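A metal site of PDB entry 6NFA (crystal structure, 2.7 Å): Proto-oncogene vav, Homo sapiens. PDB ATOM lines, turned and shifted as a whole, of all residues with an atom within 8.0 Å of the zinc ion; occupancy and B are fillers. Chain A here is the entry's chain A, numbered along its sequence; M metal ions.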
ATOM      1  N   ALA A 357      19.068 -14.394  -5.557  1.00  0.00           N
ATOM      2  CA  ALA A 357      20.268 -14.894  -4.849  1.00  0.00           C
ATOM      3  C   ALA A 357      20.667 -16.293  -5.341  1.00  0.00           C
ATOM      4  O   ALA A 357      21.851 -16.642  -5.297  1.00  0.00           O
ATOM      5  CB  ALA A 357      20.027 -14.922  -3.351  1.00  0.00           C
ATOM      6  N   ALA A 359      19.690 -17.413  -8.587  1.00  0.00           N
ATOM      7  CA  ALA A 359      19.483 -17.357 -10.031  1.00  0.00           C
ATOM      8  C   ALA A 359      20.698 -17.899 -10.801  1.00  0.00           C
ATOM      9  O   ALA A 359      21.848 -17.760 -10.359  1.00  0.00           O
ATOM     10  CB  ALA A 359      19.216 -15.926 -10.451  1.00  0.00           C
ATOM     11  N   ASN A 360      20.430 -18.539 -11.967  1.00  0.00           N
ATOM     12  CA  ASN A 360      21.407 -19.071 -12.908  1.00  0.00           C
ATOM     13  C   ASN A 360      22.497 -19.958 -12.275  1.00  0.00           C
ATOM     14  O   ASN A 360      23.677 -19.849 -12.599  1.00  0.00           O
ATOM     15  CB  ASN A 360      22.026 -17.904 -13.721  1.00  0.00           C
ATOM     16  CG  ASN A 360      20.954 -16.985 -14.317  1.00  0.00           C
ATOM     17  OD1 ASN A 360      20.898 -15.783 -14.042  1.00  0.00           O
ATOM     18  ND2 ASN A 360      20.006 -17.566 -15.043  1.00  0.00           N
ATOM     19  N   GLY A 361      22.074 -20.812 -11.333  1.00  0.00           N
ATOM     20  CA  GLY A 361      22.951 -21.734 -10.630  1.00  0.00           C
ATOM     21  C   GLY A 361      23.786 -21.178  -9.504  1.00  0.00           C
ATOM     22  O   GLY A 361      24.504 -21.925  -8.836  1.00  0.00           O
ATOM     23  N   HIS A 362      23.737 -19.863  -9.268  1.00  0.00           N
ATOM     24  CA  HIS A 362      24.566 -19.276  -8.219  1.00  0.00           C
ATOM     25  C   HIS A 362      24.000 -19.433  -6.828  1.00  0.00           C
ATOM     26  O   HIS A 362      22.824 -19.758  -6.669  1.00  0.00           O
ATOM     27  CB  HIS A 362      24.664 -17.779  -8.481  1.00  0.00           C
ATOM     28  CG  HIS A 362      25.429 -17.421  -9.702  1.00  0.00           C
ATOM     29  ND1 HIS A 362      26.809 -17.519  -9.740  1.00  0.00           N
ATOM     30  CD2 HIS A 362      24.989 -16.860 -10.839  1.00  0.00           C
ATOM     31  CE1 HIS A 362      27.169 -17.056 -10.914  1.00  0.00           C
ATOM     32  NE2 HIS A 362      26.100 -16.617 -11.611  1.00  0.00           N
ATOM     33  N   ASP A 363      24.829 -19.131  -5.807  1.00  0.00           N
ATOM     34  CA  ASP A 363      24.373 -19.033  -4.429  1.00  0.00           C
ATOM     35  C   ASP A 363      25.085 -17.847  -3.748  1.00  0.00           C
ATOM     36  O   ASP A 363      26.108 -17.992  -3.076  1.00  0.00           O
ATOM     37  CB  ASP A 363      24.427 -20.341  -3.629  1.00  0.00           C
ATOM     38  CG  ASP A 363      23.828 -20.158  -2.229  1.00  0.00           C
ATOM     39  OD1 ASP A 363      22.821 -19.419  -2.099  1.00  0.00           O
ATOM     40  OD2 ASP A 363      24.396 -20.734  -1.261  1.00  0.00           O
ATOM     41  N   PHE A 364      24.536 -16.663  -4.017  1.00  0.00           N
ATOM     42  CA  PHE A 364      25.018 -15.360  -3.538  1.00  0.00           C
ATOM     43  C   PHE A 364      24.739 -15.148  -2.094  1.00  0.00           C
ATOM     44  O   PHE A 364      23.598 -15.268  -1.667  1.00  0.00           O
ATOM     45  CB  PHE A 364      24.425 -14.220  -4.354  1.00  0.00           C
ATOM     46  CG  PHE A 364      24.978 -14.127  -5.755  1.00  0.00           C
ATOM     47  CD1 PHE A 364      26.281 -13.691  -5.973  1.00  0.00           C
ATOM     48  CD2 PHE A 364      24.194 -14.424  -6.862  1.00  0.00           C
ATOM     49  CE1 PHE A 364      26.787 -13.564  -7.271  1.00  0.00           C
ATOM     50  CE2 PHE A 364      24.703 -14.311  -8.158  1.00  0.00           C
ATOM     51  CZ  PHE A 364      26.001 -13.909  -8.352  1.00  0.00           C
ATOM     52  N   ARG A 391      28.964 -12.339  -2.882  1.00  0.00           N
ATOM     53  CA  ARG A 391      29.882 -13.277  -3.538  1.00  0.00           C
ATOM     54  C   ARG A 391      29.205 -14.666  -3.582  1.00  0.00           C
ATOM     55  O   ARG A 391      28.701 -15.128  -2.552  1.00  0.00           O
ATOM     56  CB  ARG A 391      31.247 -13.358  -2.820  1.00  0.00           C
ATOM     57  CG  ARG A 391      32.317 -14.051  -3.661  1.00  0.00           C
ATOM     58  CD  ARG A 391      33.437 -14.678  -2.832  1.00  0.00           C
ATOM     59  NE  ARG A 391      34.560 -13.770  -2.571  1.00  0.00           N
ATOM     60  CZ  ARG A 391      35.534 -13.466  -3.441  1.00  0.00           C
ATOM     61  NH1 ARG A 391      35.508 -13.958  -4.669  1.00  0.00           N
ATOM     62  NH2 ARG A 391      36.509 -12.642  -3.098  1.00  0.00           N
ATOM     63  N   CYS A 392      29.173 -15.309  -4.773  1.00  0.00           N
ATOM     64  CA  CYS A 392      28.650 -16.665  -4.914  1.00  0.00           C
ATOM     65  C   CYS A 392      29.760 -17.589  -4.411  1.00  0.00           C
ATOM     66  O   CYS A 392      30.884 -17.508  -4.917  1.00  0.00           O
ATOM     67  CB  CYS A 392      28.266 -16.993  -6.352  1.00  0.00           C
ATOM     68  SG  CYS A 392      28.115 -18.774  -6.694  1.00  0.00           S
ATOM     69  N   HIS A 393      29.479 -18.426  -3.400  1.00  0.00           N
ATOM     70  CA  HIS A 393      30.503 -19.309  -2.824  1.00  0.00           C
ATOM     71  C   HIS A 393      31.045 -20.335  -3.856  1.00  0.00           C
ATOM     72  O   HIS A 393      32.229 -20.647  -3.809  1.00  0.00           O
ATOM     73  CB  HIS A 393      30.030 -19.972  -1.521  1.00  0.00           C
ATOM     74  CG  HIS A 393      28.878 -20.915  -1.669  1.00  0.00           C
ATOM     75  ND1 HIS A 393      29.085 -22.243  -2.010  1.00  0.00           N
ATOM     76  CD2 HIS A 393      27.558 -20.698  -1.494  1.00  0.00           C
ATOM     77  CE1 HIS A 393      27.876 -22.791  -2.044  1.00  0.00           C
ATOM     78  NE2 HIS A 393      26.925 -21.906  -1.729  1.00  0.00           N
ATOM     79  N   ARG A 394      30.189 -20.772  -4.803  1.00  0.00           N
ATOM     80  CA  ARG A 394      30.497 -21.718  -5.889  1.00  0.00           C
ATOM     81  C   ARG A 394      31.570 -21.245  -6.873  1.00  0.00           C
ATOM     82  O   ARG A 394      32.604 -21.901  -6.993  1.00  0.00           O
ATOM     83  CB  ARG A 394      29.220 -22.147  -6.658  1.00  0.00           C
ATOM     84  CG  ARG A 394      28.280 -23.015  -5.867  1.00  0.00           C
ATOM     85  CD  ARG A 394      26.860 -23.043  -6.388  1.00  0.00           C
ATOM     86  NE  ARG A 394      25.990 -23.503  -5.315  1.00  0.00           N
ATOM     87  CZ  ARG A 394      24.666 -23.521  -5.355  1.00  0.00           C
ATOM     88  NH1 ARG A 394      24.021 -23.123  -6.443  1.00  0.00           N
ATOM     89  NH2 ARG A 394      23.966 -23.934  -4.304  1.00  0.00           N
ATOM     90  N   CYS A 395      31.316 -20.131  -7.598  1.00  0.00           N
ATOM     91  CA  CYS A 395      32.195 -19.568  -8.645  1.00  0.00           C
ATOM     92  C   CYS A 395      33.024 -18.354  -8.212  1.00  0.00           C
ATOM     93  O   CYS A 395      33.805 -17.851  -9.010  1.00  0.00           O
ATOM     94  CB  CYS A 395      31.362 -19.240  -9.878  1.00  0.00           C
ATOM     95  SG  CYS A 395      30.141 -17.941  -9.587  1.00  0.00           S
ATOM     96  N   ARG A 396      32.794 -17.846  -6.985  1.00  0.00           N
ATOM     97  CA  ARG A 396      33.471 -16.668  -6.397  1.00  0.00           C
ATOM     98  C   ARG A 396      33.211 -15.338  -7.196  1.00  0.00           C
ATOM     99  O   ARG A 396      33.996 -14.382  -7.071  1.00  0.00           O
ATOM    100  CB  ARG A 396      34.978 -16.940  -6.146  1.00  0.00           C
ATOM    101  CG  ARG A 396      35.260 -18.082  -5.166  1.00  0.00           C
ATOM    102  CD  ARG A 396      36.741 -18.357  -4.942  1.00  0.00           C
ATOM    103  NE  ARG A 396      37.422 -17.246  -4.267  1.00  0.00           N
ATOM    104  CZ  ARG A 396      38.324 -16.449  -4.833  1.00  0.00           C
ATOM    105  NH1 ARG A 396      38.697 -16.660  -6.093  1.00  0.00           N
ATOM    106  NH2 ARG A 396      38.868 -15.452  -4.151  1.00  0.00           N
ATOM    107  N   ALA A 397      32.107 -15.252  -7.972  1.00  0.00           N
ATOM    108  CA  ALA A 397      31.744 -14.022  -8.680  1.00  0.00           C
ATOM    109  C   ALA A 397      31.183 -12.996  -7.659  1.00  0.00           C
ATOM    110  O   ALA A 397      30.412 -13.364  -6.771  1.00  0.00           O
ATOM    111  CB  ALA A 397      30.703 -14.309  -9.780  1.00  0.00           C
ATOM    112  N   SER A 398      31.616 -11.731  -7.773  1.00  0.00           N
ATOM    113  CA  SER A 398      31.222 -10.618  -6.895  1.00  0.00           C
ATOM    114  C   SER A 398      30.138  -9.827  -7.589  1.00  0.00           C
ATOM    115  O   SER A 398      30.179  -9.740  -8.807  1.00  0.00           O
ATOM    116  CB  SER A 398      32.407  -9.697  -6.652  1.00  0.00           C
ATOM    117  OG  SER A 398      33.605 -10.416  -6.450  1.00  0.00           O
ATOM    118  N   VAL A 407      24.100 -11.410 -13.391  1.00  0.00           N
ATOM    119  CA  VAL A 407      25.419 -12.053 -13.413  1.00  0.00           C
ATOM    120  C   VAL A 407      25.432 -13.297 -14.373  1.00  0.00           C
ATOM    121  O   VAL A 407      24.388 -13.936 -14.546  1.00  0.00           O
ATOM    122  CB  VAL A 407      26.020 -12.362 -12.017  1.00  0.00           C
ATOM    123  CG1 VAL A 407      27.338 -13.143 -12.119  1.00  0.00           C
ATOM    124  CG2 VAL A 407      26.219 -11.104 -11.220  1.00  0.00           C
ATOM    125  N   PRO A 408      26.585 -13.620 -15.012  1.00  0.00           N
ATOM    126  CA  PRO A 408      26.644 -14.800 -15.912  1.00  0.00           C
ATOM    127  C   PRO A 408      26.348 -16.083 -15.139  1.00  0.00           C
ATOM    128  O   PRO A 408      26.756 -16.124 -13.983  1.00  0.00           O
ATOM    129  CB  PRO A 408      28.109 -14.839 -16.374  1.00  0.00           C
ATOM    130  CG  PRO A 408      28.646 -13.502 -16.099  1.00  0.00           C
ATOM    131  CD  PRO A 408      27.915 -12.980 -14.913  1.00  0.00           C
ATOM    132  N   PRO A 409      25.795 -17.160 -15.757  1.00  0.00           N
ATOM    133  CA  PRO A 409      25.492 -18.385 -14.977  1.00  0.00           C
ATOM    134  C   PRO A 409      26.673 -19.044 -14.264  1.00  0.00           C
ATOM    135  O   PRO A 409      27.771 -19.072 -14.814  1.00  0.00           O
ATOM    136  CB  PRO A 409      24.900 -19.331 -16.022  1.00  0.00           C
ATOM    137  CG  PRO A 409      24.363 -18.442 -17.068  1.00  0.00           C
ATOM    138  CD  PRO A 409      25.286 -17.266 -17.134  1.00  0.00           C
ATOM    139  N   CYS A 410      26.439 -19.577 -13.036  1.00  0.00           N
ATOM    140  CA  CYS A 410      27.443 -20.272 -12.216  1.00  0.00           C
ATOM    141  C   CYS A 410      28.089 -21.445 -12.988  1.00  0.00           C
ATOM    142  O   CYS A 410      27.373 -22.246 -13.601  1.00  0.00           O
ATOM    143  CB  CYS A 410      26.841 -20.714 -10.889  1.00  0.00           C
ATOM    144  SG  CYS A 410      28.059 -21.117  -9.631  1.00  0.00           S
ATOM    145  N   GLY A 411      29.424 -21.471 -13.006  1.00  0.00           N
ATOM    146  CA  GLY A 411      30.230 -22.468 -13.714  1.00  0.00           C
ATOM    147  C   GLY A 411      30.093 -22.360 -15.223  1.00  0.00           C
ATOM    148  O   GLY A 411      29.575 -23.291 -15.856  1.00  0.00           O
ATOM    149  N   ARG A 412      30.509 -21.183 -15.780  1.00  0.00           N
ATOM    150  CA  ARG A 412      30.469 -20.832 -17.208  1.00  0.00           C
ATOM    151  C   ARG A 412      31.335 -21.836 -18.012  1.00  0.00           C
ATOM    152  O   ARG A 412      31.905 -21.552 -19.068  1.00  0.00           O
ATOM    153  CB  ARG A 412      30.912 -19.363 -17.406  1.00  0.00           C
HETATM  154 ZN    ZN M   1      28.131 -18.731  -9.013  1.00  0.00          ZN
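A ring nitrogen (ND1) of His 362 is bound to the zinc ion (1.9 Å). The zinc ion is bound by SG of Cys 395 (2.2 Å). The side-chain sulfur (SG) of Cys 392 is bound to the zinc ion (2.3 Å). The zinc ion is bound by the side-chain sulfur (SG) of Cys 410, 2.5 Å away.
NE2 of His 362 lies within hydrogen-bond range of O of Pro 408 (2.5 Å). The side-chain sulfur of Cys 395 lies close to the backbone NH of Ala 397 (3.7 Å). SG of Cys 392 lies close to N of Arg 394 (3.4 Å). The side-chain sulfur (SG) of Cys 392 sits close to the backbone NH (N) of Asp 363. N of Cys 392 is in hydrogen-bond range of O of Ala 397. The backbone carbonyl oxygen (O) of Gly 361 sits close to the side-chain sulfur (SG) of Cys 410 (3.7 Å). The backbone NH of Cys 410 is in hydrogen-bond range of the backbone carbonyl oxygen of Asn 360, 2.8 Å away.
Of the 21 residues printed, 4 come within 4 Å of the zinc ion.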
